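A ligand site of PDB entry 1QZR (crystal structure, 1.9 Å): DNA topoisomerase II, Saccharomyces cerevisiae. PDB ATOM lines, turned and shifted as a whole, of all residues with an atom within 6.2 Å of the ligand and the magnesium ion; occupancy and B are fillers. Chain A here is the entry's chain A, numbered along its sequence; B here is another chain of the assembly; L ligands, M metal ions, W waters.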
ATOM      1  N   GLU A  71      11.492 -10.073  19.809  1.00  0.00           N
ATOM      2  CA  GLU A  71      11.854 -10.502  21.148  1.00  0.00           C
ATOM      3  C   GLU A  71      10.731 -11.366  21.762  1.00  0.00           C
ATOM      4  O   GLU A  71      10.996 -12.401  22.382  1.00  0.00           O
ATOM      5  CB  GLU A  71      12.172  -9.303  22.064  1.00  0.00           C
ATOM      6  CG  GLU A  71      13.465  -8.557  21.704  1.00  0.00           C
ATOM      7  CD  GLU A  71      14.754  -9.273  22.141  1.00  0.00           C
ATOM      8  OE1 GLU A  71      14.715 -10.457  22.575  1.00  0.00           O
ATOM      9  OE2 GLU A  71      15.852  -8.644  22.046  1.00  0.00           O
ATOM     10  N   ILE A  72       9.495 -10.958  21.533  1.00  0.00           N
ATOM     11  CA  ILE A  72       8.336 -11.681  22.121  1.00  0.00           C
ATOM     12  C   ILE A  72       8.107 -13.001  21.383  1.00  0.00           C
ATOM     13  O   ILE A  72       7.774 -14.024  22.010  1.00  0.00           O
ATOM     14  CB  ILE A  72       7.075 -10.800  22.113  1.00  0.00           C
ATOM     15  CG1 ILE A  72       7.307  -9.526  22.952  1.00  0.00           C
ATOM     16  CG2 ILE A  72       5.829 -11.564  22.643  1.00  0.00           C
ATOM     17  CD1 ILE A  72       7.878  -9.770  24.363  1.00  0.00           C
ATOM     18  N   VAL A  74      10.386 -14.862  19.806  1.00  0.00           N
ATOM     19  CA  VAL A  74      11.444 -15.796  20.160  1.00  0.00           C
ATOM     20  C   VAL A  74      11.257 -16.379  21.565  1.00  0.00           C
ATOM     21  O   VAL A  74      11.546 -17.560  21.778  1.00  0.00           O
ATOM     22  CB  VAL A  74      12.846 -15.164  19.966  1.00  0.00           C
ATOM     23  CG1 VAL A  74      13.939 -16.093  20.502  1.00  0.00           C
ATOM     24  CG2 VAL A  74      13.085 -14.898  18.473  1.00  0.00           C
ATOM     25  N   ASN A  75      10.760 -15.570  22.508  1.00  0.00           N
ATOM     26  CA  ASN A  75      10.371 -16.089  23.849  1.00  0.00           C
ATOM     27  C   ASN A  75       9.340 -17.186  23.762  1.00  0.00           C
ATOM     28  O   ASN A  75       9.401 -18.173  24.497  1.00  0.00           O
ATOM     29  CB  ASN A  75       9.849 -14.952  24.760  1.00  0.00           C
ATOM     30  CG  ASN A  75      10.960 -14.062  25.285  1.00  0.00           C
ATOM     31  OD1 ASN A  75      12.145 -14.431  25.222  1.00  0.00           O
ATOM     32  ND2 ASN A  75      10.603 -12.885  25.796  1.00  0.00           N
ATOM     33  N   ALA A  76       8.378 -17.025  22.865  1.00  0.00           N
ATOM     34  CA  ALA A  76       7.351 -18.046  22.678  1.00  0.00           C
ATOM     35  C   ALA A  76       7.942 -19.317  22.095  1.00  0.00           C
ATOM     36  O   ALA A  76       7.658 -20.426  22.573  1.00  0.00           O
ATOM     37  CB  ALA A  76       6.209 -17.517  21.810  1.00  0.00           C
ATOM     38  N   ASP A  78      10.995 -20.218  22.453  1.00  0.00           N
ATOM     39  CA  ASP A  78      11.810 -20.780  23.531  1.00  0.00           C
ATOM     40  C   ASP A  78      10.998 -21.699  24.434  1.00  0.00           C
ATOM     41  O   ASP A  78      11.558 -22.622  25.030  1.00  0.00           O
ATOM     42  CB  ASP A  78      12.470 -19.666  24.373  1.00  0.00           C
ATOM     43  CG  ASP A  78      13.636 -19.000  23.654  1.00  0.00           C
ATOM     44  OD1 ASP A  78      14.163 -19.613  22.686  1.00  0.00           O
ATOM     45  OD2 ASP A  78      14.084 -17.865  23.952  1.00  0.00           O
ATOM     46  N   ASN A  79       9.695 -21.458  24.530  1.00  0.00           N
ATOM     47  CA  ASN A  79       8.852 -22.285  25.387  1.00  0.00           C
ATOM     48  C   ASN A  79       8.697 -23.707  24.879  1.00  0.00           C
ATOM     49  O   ASN A  79       8.438 -24.618  25.658  1.00  0.00           O
ATOM     50  CB  ASN A  79       7.478 -21.653  25.634  1.00  0.00           C
ATOM     51  CG  ASN A  79       6.845 -22.134  26.930  1.00  0.00           C
ATOM     52  OD1 ASN A  79       7.442 -22.003  27.995  1.00  0.00           O
ATOM     53  ND2 ASN A  79       5.661 -22.720  26.848  1.00  0.00           N
ATOM     54  N   ARG A  82      11.646 -25.582  26.543  1.00  0.00           N
ATOM     55  CA  ARG A  82      11.314 -25.888  27.948  1.00  0.00           C
ATOM     56  C   ARG A  82      10.124 -26.857  28.087  1.00  0.00           C
ATOM     57  O   ARG A  82      10.109 -27.708  28.983  1.00  0.00           O
ATOM     58  CB  ARG A  82      11.118 -24.581  28.735  1.00  0.00           C
ATOM     59  CG  ARG A  82       9.916 -24.471  29.674  1.00  0.00           C
ATOM     60  CD  ARG A  82       9.732 -23.040  30.215  1.00  0.00           C
ATOM     61  NE  ARG A  82       9.145 -22.963  31.547  1.00  0.00           N
ATOM     62  CZ  ARG A  82       7.918 -22.509  31.790  1.00  0.00           C
ATOM     63  NH1 ARG A  82       7.127 -22.148  30.793  1.00  0.00           N
ATOM     64  NH2 ARG A  82       7.465 -22.444  33.032  1.00  0.00           N
ATOM     65  N   ASN A 104       1.213 -18.466  23.432  1.00  0.00           N
ATOM     66  CA  ASN A 104       1.685 -19.817  23.258  1.00  0.00           C
ATOM     67  C   ASN A 104       1.028 -20.721  24.263  1.00  0.00           C
ATOM     68  O   ASN A 104       0.647 -20.286  25.356  1.00  0.00           O
ATOM     69  CB  ASN A 104       3.222 -19.860  23.367  1.00  0.00           C
ATOM     70  CG  ASN A 104       3.732 -19.433  24.745  1.00  0.00           C
ATOM     71  OD1 ASN A 104       4.098 -18.285  24.952  1.00  0.00           O
ATOM     72  ND2 ASN A 104       3.739 -20.374  25.689  1.00  0.00           N
ATOM     73  N   LYS A 107       3.523 -25.035  29.046  1.00  0.00           N
ATOM     74  CA  LYS A 107       3.755 -24.509  30.396  1.00  0.00           C
ATOM     75  C   LYS A 107       3.726 -22.978  30.432  1.00  0.00           C
ATOM     76  O   LYS A 107       4.364 -22.339  29.609  1.00  0.00           O
ATOM     77  CB  LYS A 107       5.097 -25.010  30.930  1.00  0.00           C
ATOM     78  CG  LYS A 107       5.243 -24.919  32.439  1.00  0.00           C
ATOM     79  CD  LYS A 107       6.336 -25.849  32.974  1.00  0.00           C
ATOM     80  CE  LYS A 107       6.809 -25.413  34.361  1.00  0.00           C
ATOM     81  NZ  LYS A 107       6.805 -26.530  35.347  1.00  0.00           N
ATOM     82  N   GLY A 108       2.957 -22.422  31.371  1.00  0.00           N
ATOM     83  CA  GLY A 108       2.941 -20.978  31.588  1.00  0.00           C
ATOM     84  C   GLY A 108       4.048 -20.543  32.543  1.00  0.00           C
ATOM     85  O   GLY A 108       5.000 -21.299  32.766  1.00  0.00           O
ATOM     86  N   ILE A 109       3.940 -19.321  33.078  1.00  0.00           N
ATOM     87  CA  ILE A 109       4.899 -18.799  34.078  1.00  0.00           C
ATOM     88  C   ILE A 109       4.403 -19.131  35.487  1.00  0.00           C
ATOM     89  O   ILE A 109       3.245 -18.927  35.785  1.00  0.00           O
ATOM     90  CB  ILE A 109       5.056 -17.237  33.979  1.00  0.00           C
ATOM     91  CG1 ILE A 109       5.017 -16.707  32.523  1.00  0.00           C
ATOM     92  CG2 ILE A 109       6.294 -16.742  34.765  1.00  0.00           C
ATOM     93  CD1 ILE A 109       6.196 -17.035  31.697  1.00  0.00           C
ATOM     94  N   ILE A 125      10.179 -11.048  36.011  1.00  0.00           N
ATOM     95  CA  ILE A 125      10.840 -11.370  34.746  1.00  0.00           C
ATOM     96  C   ILE A 125      10.324 -10.604  33.529  1.00  0.00           C
ATOM     97  O   ILE A 125      10.941 -10.633  32.449  1.00  0.00           O
ATOM     98  CB  ILE A 125      10.862 -12.913  34.522  1.00  0.00           C
ATOM     99  CG1 ILE A 125       9.447 -13.435  34.208  1.00  0.00           C
ATOM    100  CG2 ILE A 125      11.453 -13.597  35.749  1.00  0.00           C
ATOM    101  CD1 ILE A 125       9.400 -14.925  33.864  1.00  0.00           C
ATOM    102  N   PHE A 126       9.190  -9.899  33.693  1.00  0.00           N
ATOM    103  CA  PHE A 126       8.687  -9.011  32.629  1.00  0.00           C
ATOM    104  C   PHE A 126       8.783  -7.520  32.956  1.00  0.00           C
ATOM    105  O   PHE A 126       8.618  -6.677  32.063  1.00  0.00           O
ATOM    106  CB  PHE A 126       7.238  -9.362  32.268  1.00  0.00           C
ATOM    107  CG  PHE A 126       7.111 -10.609  31.445  1.00  0.00           C
ATOM    108  CD1 PHE A 126       7.169 -10.557  30.070  1.00  0.00           C
ATOM    109  CD2 PHE A 126       6.926 -11.840  32.057  1.00  0.00           C
ATOM    110  CE1 PHE A 126       7.070 -11.726  29.284  1.00  0.00           C
ATOM    111  CE2 PHE A 126       6.810 -13.011  31.294  1.00  0.00           C
ATOM    112  CZ  PHE A 126       6.888 -12.951  29.908  1.00  0.00           C
ATOM    113  N   THR A 131      16.698 -10.113  34.327  1.00  0.00           N
ATOM    114  CA  THR A 131      15.989 -11.229  34.932  1.00  0.00           C
ATOM    115  C   THR A 131      15.810 -12.281  33.879  1.00  0.00           C
ATOM    116  O   THR A 131      15.379 -11.973  32.763  1.00  0.00           O
ATOM    117  CB  THR A 131      14.619 -10.783  35.465  1.00  0.00           C
ATOM    118  OG1 THR A 131      13.929 -10.060  34.442  1.00  0.00           O
ATOM    119  CG2 THR A 131      14.761  -9.774  36.583  1.00  0.00           C
ATOM    120  N   SER A 132      16.107 -13.522  34.229  1.00  0.00           N
ATOM    121  CA  SER A 132      16.152 -14.592  33.243  1.00  0.00           C
ATOM    122  C   SER A 132      16.167 -15.958  33.902  1.00  0.00           C
ATOM    123  O   SER A 132      16.590 -16.091  35.032  1.00  0.00           O
ATOM    124  CB  SER A 132      17.410 -14.442  32.364  1.00  0.00           C
ATOM    125  OG  SER A 132      17.390 -15.402  31.311  1.00  0.00           O
ATOM    126  N   SER A 133      15.716 -16.962  33.157  1.00  0.00           N
ATOM    127  CA  SER A 133      15.925 -18.367  33.522  1.00  0.00           C
ATOM    128  C   SER A 133      17.142 -18.935  32.781  1.00  0.00           C
ATOM    129  O   SER A 133      17.423 -20.130  32.848  1.00  0.00           O
ATOM    130  CB  SER A 133      14.667 -19.186  33.188  1.00  0.00           C
ATOM    131  OG  SER A 133      14.403 -19.135  31.796  1.00  0.00           O
ATOM    132  N   ASN A 134      17.871 -18.065  32.067  1.00  0.00           N
ATOM    133  CA  ASN A 134      18.970 -18.524  31.213  1.00  0.00           C
ATOM    134  C   ASN A 134      20.362 -18.159  31.718  1.00  0.00           C
ATOM    135  O   ASN A 134      21.309 -18.130  30.936  1.00  0.00           O
ATOM    136  CB  ASN A 134      18.775 -18.005  29.775  1.00  0.00           C
ATOM    137  CG  ASN A 134      17.588 -18.649  29.087  1.00  0.00           C
ATOM    138  OD1 ASN A 134      16.597 -17.968  28.732  1.00  0.00           O
ATOM    139  ND2 ASN A 134      17.667 -19.945  28.896  1.00  0.00           N
ATOM    140  N   GLY A 144      16.826 -19.569  22.517  1.00  0.00           N
ATOM    141  CA  GLY A 144      17.302 -18.291  22.010  1.00  0.00           C
ATOM    142  C   GLY A 144      17.599 -17.283  23.115  1.00  0.00           C
ATOM    143  O   GLY A 144      18.480 -16.426  22.947  1.00  0.00           O
ATOM    144  N   GLY A 145      16.897 -17.399  24.249  1.00  0.00           N
ATOM    145  CA  GLY A 145      17.083 -16.437  25.332  1.00  0.00           C
ATOM    146  C   GLY A 145      18.421 -16.583  26.026  1.00  0.00           C
ATOM    147  O   GLY A 145      18.824 -17.703  26.343  1.00  0.00           O
ATOM    148  N   ARG A 146      19.095 -15.456  26.265  1.00  0.00           N
ATOM    149  CA  ARG A 146      20.452 -15.457  26.807  1.00  0.00           C
ATOM    150  C   ARG A 146      20.696 -14.394  27.898  1.00  0.00           C
ATOM    151  O   ARG A 146      21.284 -14.713  28.931  1.00  0.00           O
ATOM    152  CB  ARG A 146      21.503 -15.271  25.691  1.00  0.00           C
ATOM    153  CG  ARG A 146      21.555 -16.404  24.625  1.00  0.00           C
ATOM    154  CD  ARG A 146      22.028 -17.765  25.162  1.00  0.00           C
ATOM    155  NE  ARG A 146      23.397 -17.697  25.686  1.00  0.00           N
ATOM    156  CZ  ARG A 146      23.777 -18.155  26.869  1.00  0.00           C
ATOM    157  NH1 ARG A 146      22.891 -18.751  27.671  1.00  0.00           N
ATOM    158  NH2 ARG A 146      25.029 -18.050  27.263  1.00  0.00           N
ATOM    159  N   ASN A 147      20.228 -13.168  27.687  1.00  0.00           N
ATOM    160  CA  ASN A 147      20.668 -12.018  28.501  1.00  0.00           C
ATOM    161  C   ASN A 147      19.710 -11.470  29.541  1.00  0.00           C
ATOM    162  O   ASN A 147      20.132 -10.693  30.430  1.00  0.00           O
ATOM    163  CB  ASN A 147      21.099 -10.879  27.600  1.00  0.00           C
ATOM    164  CG  ASN A 147      22.134 -11.306  26.584  1.00  0.00           C
ATOM    165  OD1 ASN A 147      23.122 -11.951  26.932  1.00  0.00           O
ATOM    166  ND2 ASN A 147      21.912 -10.950  25.326  1.00  0.00           N
ATOM    167  N   GLY A 148      18.437 -11.817  29.425  1.00  0.00           N
ATOM    168  CA  GLY A 148      17.434 -11.306  30.361  1.00  0.00           C
ATOM    169  C   GLY A 148      17.021  -9.869  30.126  1.00  0.00           C
ATOM    170  O   GLY A 148      16.671  -9.166  31.081  1.00  0.00           O
ATOM    171  N   TYR A 149      17.000  -9.451  28.851  1.00  0.00           N
ATOM    172  CA  TYR A 149      16.580  -8.099  28.453  1.00  0.00           C
ATOM    173  C   TYR A 149      15.344  -8.071  27.557  1.00  0.00           C
ATOM    174  O   TYR A 149      14.538  -7.145  27.638  1.00  0.00           O
ATOM    175  CB  TYR A 149      17.714  -7.399  27.698  1.00  0.00           C
ATOM    176  CG  TYR A 149      18.710  -6.697  28.590  1.00  0.00           C
ATOM    177  CD1 TYR A 149      19.797  -7.382  29.123  1.00  0.00           C
ATOM    178  CD2 TYR A 149      18.543  -5.345  28.924  1.00  0.00           C
ATOM    179  CE1 TYR A 149      20.740  -6.735  29.936  1.00  0.00           C
ATOM    180  CE2 TYR A 149      19.452  -4.684  29.759  1.00  0.00           C
ATOM    181  CZ  TYR A 149      20.557  -5.398  30.267  1.00  0.00           C
ATOM    182  OH  TYR A 149      21.463  -4.772  31.078  1.00  0.00           O
ATOM    183  N   GLY A 150      15.230  -9.071  26.676  1.00  0.00           N
ATOM    184  CA  GLY A 150      14.236  -9.081  25.598  1.00  0.00           C
ATOM    185  C   GLY A 150      12.824  -8.577  25.900  1.00  0.00           C
ATOM    186  O   GLY A 150      12.373  -7.601  25.307  1.00  0.00           O
ATOM    187  N   ALA A 151      12.133  -9.232  26.822  1.00  0.00           N
ATOM    188  CA  ALA A 151      10.758  -8.873  27.159  1.00  0.00           C
ATOM    189  C   ALA A 151      10.633  -7.488  27.813  1.00  0.00           C
ATOM    190  O   ALA A 151       9.663  -6.773  27.599  1.00  0.00           O
ATOM    191  CB  ALA A 151      10.140  -9.965  28.030  1.00  0.00           C
ATOM    192  N   LYS A 152      11.631  -7.115  28.598  1.00  0.00           N
ATOM    193  CA  LYS A 152      11.643  -5.798  29.227  1.00  0.00           C
ATOM    194  C   LYS A 152      11.872  -4.702  28.189  1.00  0.00           C
ATOM    195  O   LYS A 152      11.310  -3.619  28.294  1.00  0.00           O
ATOM    196  CB  LYS A 152      12.720  -5.720  30.319  1.00  0.00           C
ATOM    197  CG  LYS A 152      12.276  -6.301  31.667  1.00  0.00           C
ATOM    198  CD  LYS A 152      12.183  -7.833  31.649  1.00  0.00           C
ATOM    199  CE  LYS A 152      13.591  -8.499  31.535  1.00  0.00           C
ATOM    200  NZ  LYS A 152      13.484  -9.995  31.554  1.00  0.00           N
ATOM    201  N   LEU A 153      12.699  -4.985  27.174  1.00  0.00           N
ATOM    202  CA  LEU A 153      12.898  -4.021  26.099  1.00  0.00           C
ATOM    203  C   LEU A 153      11.592  -3.766  25.345  1.00  0.00           C
ATOM    204  O   LEU A 153      11.278  -2.641  24.995  1.00  0.00           O
ATOM    205  CB  LEU A 153      14.016  -4.458  25.131  1.00  0.00           C
ATOM    206  CG  LEU A 153      15.416  -4.460  25.764  1.00  0.00           C
ATOM    207  CD1 LEU A 153      16.473  -5.035  24.807  1.00  0.00           C
ATOM    208  CD2 LEU A 153      15.838  -3.049  26.249  1.00  0.00           C
ATOM    209  N   THR A 200       0.601 -18.736  27.948  1.00  0.00           N
ATOM    210  CA  THR A 200       1.048 -17.390  28.209  1.00  0.00           C
ATOM    211  C   THR A 200       0.669 -16.522  27.022  1.00  0.00           C
ATOM    212  O   THR A 200       0.819 -16.928  25.866  1.00  0.00           O
ATOM    213  CB  THR A 200       2.559 -17.385  28.427  1.00  0.00           C
ATOM    214  OG1 THR A 200       2.855 -18.060  29.647  1.00  0.00           O
ATOM    215  CG2 THR A 200       3.086 -15.947  28.668  1.00  0.00           C
ATOM    216  N   VAL A 202       1.123 -12.498  25.700  1.00  0.00           N
ATOM    217  CA  VAL A 202       1.725 -11.169  25.833  1.00  0.00           C
ATOM    218  C   VAL A 202       1.034 -10.256  24.841  1.00  0.00           C
ATOM    219  O   VAL A 202       0.954 -10.578  23.655  1.00  0.00           O
ATOM    220  CB  VAL A 202       3.271 -11.214  25.549  1.00  0.00           C
ATOM    221  CG1 VAL A 202       3.858  -9.790  25.483  1.00  0.00           C
ATOM    222  CG2 VAL A 202       4.009 -12.044  26.611  1.00  0.00           C
ATOM    223  N   GLN A 370      22.679  -7.438  21.580  1.00  0.00           N
ATOM    224  CA  GLN A 370      21.376  -7.873  22.074  1.00  0.00           C
ATOM    225  C   GLN A 370      20.426  -8.264  20.939  1.00  0.00           C
ATOM    226  O   GLN A 370      19.574  -9.118  21.136  1.00  0.00           O
ATOM    227  CB  GLN A 370      20.732  -6.791  22.971  1.00  0.00           C
ATOM    228  CG  GLN A 370      19.298  -7.133  23.445  1.00  0.00           C
ATOM    229  CD  GLN A 370      19.228  -8.384  24.334  1.00  0.00           C
ATOM    230  OE1 GLN A 370      20.133  -8.649  25.102  1.00  0.00           O
ATOM    231  NE2 GLN A 370      18.130  -9.125  24.234  1.00  0.00           N
ATOM    232  N   LYS A 372      21.113  -9.934  18.322  1.00  0.00           N
ATOM    233  CA  LYS A 372      21.455 -11.315  17.907  1.00  0.00           C
ATOM    234  C   LYS A 372      21.418 -11.530  16.399  1.00  0.00           C
ATOM    235  O   LYS A 372      21.025 -12.596  15.914  1.00  0.00           O
ATOM    236  CB  LYS A 372      20.570 -12.344  18.616  1.00  0.00           C
ATOM    237  CG  LYS A 372      20.681 -12.322  20.135  1.00  0.00           C
ATOM    238  CD  LYS A 372      19.559 -13.116  20.766  1.00  0.00           C
ATOM    239  CE  LYS A 372      19.657 -13.101  22.284  1.00  0.00           C
ATOM    240  NZ  LYS A 372      19.658 -11.739  22.824  1.00  0.00           N
ATOM    241  N   TYR B  17      14.465 -18.829  38.168  1.00  0.00           N
ATOM    242  CA  TYR B  17      14.535 -17.434  37.703  1.00  0.00           C
ATOM    243  C   TYR B  17      15.440 -16.581  38.591  1.00  0.00           C
ATOM    244  O   TYR B  17      15.318 -16.618  39.820  1.00  0.00           O
ATOM    245  CB  TYR B  17      13.135 -16.819  37.601  1.00  0.00           C
ATOM    246  CG  TYR B  17      12.162 -17.631  36.782  1.00  0.00           C
ATOM    247  CD1 TYR B  17      12.074 -17.460  35.389  1.00  0.00           C
ATOM    248  CD2 TYR B  17      11.362 -18.578  37.369  1.00  0.00           C
ATOM    249  CE1 TYR B  17      11.172 -18.217  34.635  1.00  0.00           C
ATOM    250  CE2 TYR B  17      10.461 -19.339  36.625  1.00  0.00           C
ATOM    251  CZ  TYR B  17      10.383 -19.161  35.265  1.00  0.00           C
ATOM    252  OH  TYR B  17       9.498 -19.922  34.540  1.00  0.00           O
HETATM  253  P1  LIG L   1      17.123 -12.393  26.063  1.00  0.00           P
HETATM  254  O1  LIG L   1      17.278 -10.984  26.544  1.00  0.00           O
HETATM  255  O2  LIG L   1      15.873 -12.496  25.237  1.00  0.00           O
HETATM  256  O3  LIG L   1      18.313 -12.773  25.248  1.00  0.00           O
HETATM  257  P2  LIG L   1      15.590 -14.013  27.984  1.00  0.00           P
HETATM  258  O4  LIG L   1      14.681 -14.625  26.973  1.00  0.00           O
HETATM  259  O5  LIG L   1      15.967 -15.036  29.014  1.00  0.00           O
HETATM  260  N1  LIG L   1      17.023 -13.459  27.343  1.00  0.00           N
HETATM  261  P3  LIG L   1      13.543 -12.220  28.373  1.00  0.00           P
HETATM  262  O6  LIG L   1      13.200 -12.180  26.923  1.00  0.00           O
HETATM  263  O7  LIG L   1      13.502 -10.830  28.930  1.00  0.00           O
HETATM  264  O8  LIG L   1      14.932 -12.791  28.645  1.00  0.00           O
HETATM  265  O9  LIG L   1      12.532 -13.069  29.127  1.00  0.00           O
HETATM  266  C1  LIG L   1      12.645 -13.155  30.540  1.00  0.00           C
HETATM  267  C2  LIG L   1      12.329 -14.563  31.048  1.00  0.00           C
HETATM  268  O10 LIG L   1      10.935 -14.755  30.978  1.00  0.00           O
HETATM  269  C3  LIG L   1      12.884 -15.676  30.163  1.00  0.00           C
HETATM  270  O11 LIG L   1      14.139 -16.114  30.626  1.00  0.00           O
HETATM  271  C4  LIG L   1      11.851 -16.792  30.264  1.00  0.00           C
HETATM  272  O12 LIG L   1      12.162 -17.562  31.424  1.00  0.00           O
HETATM  273  C5  LIG L   1      10.563 -16.061  30.592  1.00  0.00           C
HETATM  274  N2  LIG L   1       9.616 -16.004  29.468  1.00  0.00           N
HETATM  275  C6  LIG L   1       9.456 -14.984  28.599  1.00  0.00           C
HETATM  276  N3  LIG L   1       8.462 -15.251  27.725  1.00  0.00           N
HETATM  277  C7  LIG L   1       7.992 -16.472  28.025  1.00  0.00           C
HETATM  278  C8  LIG L   1       6.934 -17.355  27.495  1.00  0.00           C
HETATM  279  N4  LIG L   1       6.185 -16.968  26.383  1.00  0.00           N
HETATM  280  N5  LIG L   1       6.736 -18.546  28.102  1.00  0.00           N
HETATM  281  C9  LIG L   1       7.473 -18.933  29.162  1.00  0.00           C
HETATM  282  N6  LIG L   1       8.450 -18.171  29.701  1.00  0.00           N
HETATM  283  C10 LIG L   1       8.737 -16.958  29.175  1.00  0.00           C
HETATM  284 MG    MG M   1      14.024 -13.425  25.491  1.00  0.00          MG
HETATM  285  O   HOH W   1       7.653 -12.958  26.159  1.00  0.00           O
HETATM  286  O   HOH W   2      12.014 -20.592  31.385  1.00  0.00           O
HETATM  287  O   HOH W   3      14.678 -14.785  23.910  1.00  0.00           O
HETATM  288  O   HOH W   4      16.250 -13.403  22.032  1.00  0.00           O
HETATM  289  O   HOH W   5      13.493 -17.011  26.767  1.00  0.00           O
HETATM  290  O   HOH W   6      10.119 -20.403  27.974  1.00  0.00           O
HETATM  291  O   HOH W   7      13.292 -12.142  23.966  1.00  0.00           O
HETATM  292  O   HOH W   8       6.376 -14.776  24.335  1.00  0.00           O
HETATM  293  O   HOH W   9       9.592 -19.575  31.811  1.00  0.00           O
HETATM  294  O   HOH W  10      10.672 -17.931  26.966  1.00  0.00           O
HETATM  295  O   HOH W  11       4.419 -19.966  28.518  1.00  0.00           O
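OG of Ser 132 lies within hydrogen-bond range of O5 of the ligand (2.7 Å). The side-chain amino group (NZ) of Lys 152 lies within salt-bridge range of an oxygen (O7) of the ligand (2.8 Å). The backbone NH (N) of Ser 133 sits at hydrogen-bond distance from an oxygen (O11) of the ligand (3.1 Å). The side-chain hydroxyl of Ser 133 lies within hydrogen-bond range of an oxygen (O12) of the ligand (2.8 Å). N of Tyr 149 lies within hydrogen-bond range of O1 of the ligand (2.8 Å). N of Gly 150 sits at hydrogen-bond distance from O1 of the ligand, at 2.8 Å. The side-chain amide oxygen (OD1) of Asn 104 is in hydrogen-bond range of a nitrogen (N4) of the ligand (2.9 Å). The side-chain amino group (NZ) of Lys 372 lies within salt-bridge range of an oxygen (O3) of the ligand (3.0 Å). An oxygen (O3) of the ligand sits at hydrogen-bond distance from the backbone NH (N) of Arg 146 (3.0 Å). O7 of the ligand lies within hydrogen-bond range of N of Ala 151, 3.0 Å away. An oxygen (O1) of the ligand lies within hydrogen-bond range of the backbone NH (N) of Gly 148 (3.2 Å). O5 of the ligand sits close to OD1 of Asn 134 (3.0 Å). The side-chain amide nitrogen (NE2) of Gln 370 is in hydrogen-bond range of an oxygen (O1) of the ligand (3.1 Å). O3 of the ligand lies within hydrogen-bond range of N of Asn 147 (3.1 Å).
The side-chain amino group (NZ) of Lys 152 sits close to the backbone carbonyl oxygen (O) of Gly 148, 3.3 Å away. O of Ile 125 sits at hydrogen-bond distance from NZ of Lys 152 (2.8 Å). ND2 of Asn 104 lies close to ND2 of Asn 79, at 3.2 Å. The side-chain amide nitrogen of Asn 147 sits close to the side-chain amino group of Lys 372 (3.5 Å). O of Gly 148 is in hydrogen-bond range of N of Thr 131, at 3.4 Å. The side-chain amide nitrogen (ND2) of Asn 147 sits at hydrogen-bond distance from the side-chain amide oxygen (OE1) of Gln 370. NH1 of Arg 82 sits at hydrogen-bond distance from OD1 of Asn 79, 2.8 Å away. ND2 of Asn 79 lies within hydrogen-bond range of O of Lys 107 (3.1 Å).
Merely in contact with the ligand: Ile 109 (3.2 Å), Ile 125 (3.3 Å), Asn 79 (3.3 Å), Tyr 17 of chain B (3.4 Å), Gly 145 (3.4 Å), Phe 126 (3.5 Å), Glu 71 (3.5 Å), Arg 82 (3.6 Å), Thr 131 (3.7 Å) and Thr 200 (3.98 Å). Hydrophobic or aromatic side chains within 4 Å of the ligand: Ile 109, Ile 125, Phe 126, Tyr 149, Ala 151 and Tyr 17 of chain B. 24 residues have an atom within 4 Å of the ligand: Glu 71, Asn 75, Asn 79, Arg 82, Asn 104, Ile 109, Ile 125, Phe 126, Thr 131, Ser 132, Ser 133, Asn 134, Gly 145, Arg 146, Asn 147, Gly 148, Tyr 149, Gly 150, Ala 151, Lys 152, Thr 200, Gln 370, Lys 372 and Tyr 17 of chain B. The nearest printed residue that does not touch the ligand is Ala 76 (4.03 Å).
One residue has an atom within 4 Å of the magnesium ion: Asn 75.
The magnesium ion is bound by O4 of the ligand (2.0 Å), O6 of the ligand (2.1 Å), O2 of the ligand (2.1 Å), water W7 (2.1 Å), OD1 of Asn 75 (2.1 Å) and water W3 (2.2 Å).
Water W7 bridges the side-chain carboxylate (OE1) of Glu 71 (2.6 Å) and the side-chain amide nitrogen (ND2) of Asn 75 (3.3 Å). Water W3 lies within hydrogen-bond range of OD2 of Asp 78 (3.1 Å) and N of Gly 145 (3.4 Å). Water W11 lies within hydrogen-bond range of the backbone carbonyl oxygen of Lys 107, the side-chain hydroxyl of Thr 200, a nitrogen (N5) of the ligand, the side-chain amide nitrogen of Asn 104 and the side-chain amide nitrogen of Asn 79. Water W9 lies within hydrogen-bond range of the side-chain hydroxyl of Tyr 17 of chain B (2.8 Å), a nitrogen (N6) of the ligand (2.8 Å) and the guanidinium group of Arg 82 (3.4 Å). Water W1 lies within hydrogen-bond range of N3 of the ligand (2.9 Å) and ND2 of Asn 75 (3.0 Å). Water W2 bridges OG of Ser 133 (2.8 Å) and O12 of the ligand (3.0 Å).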
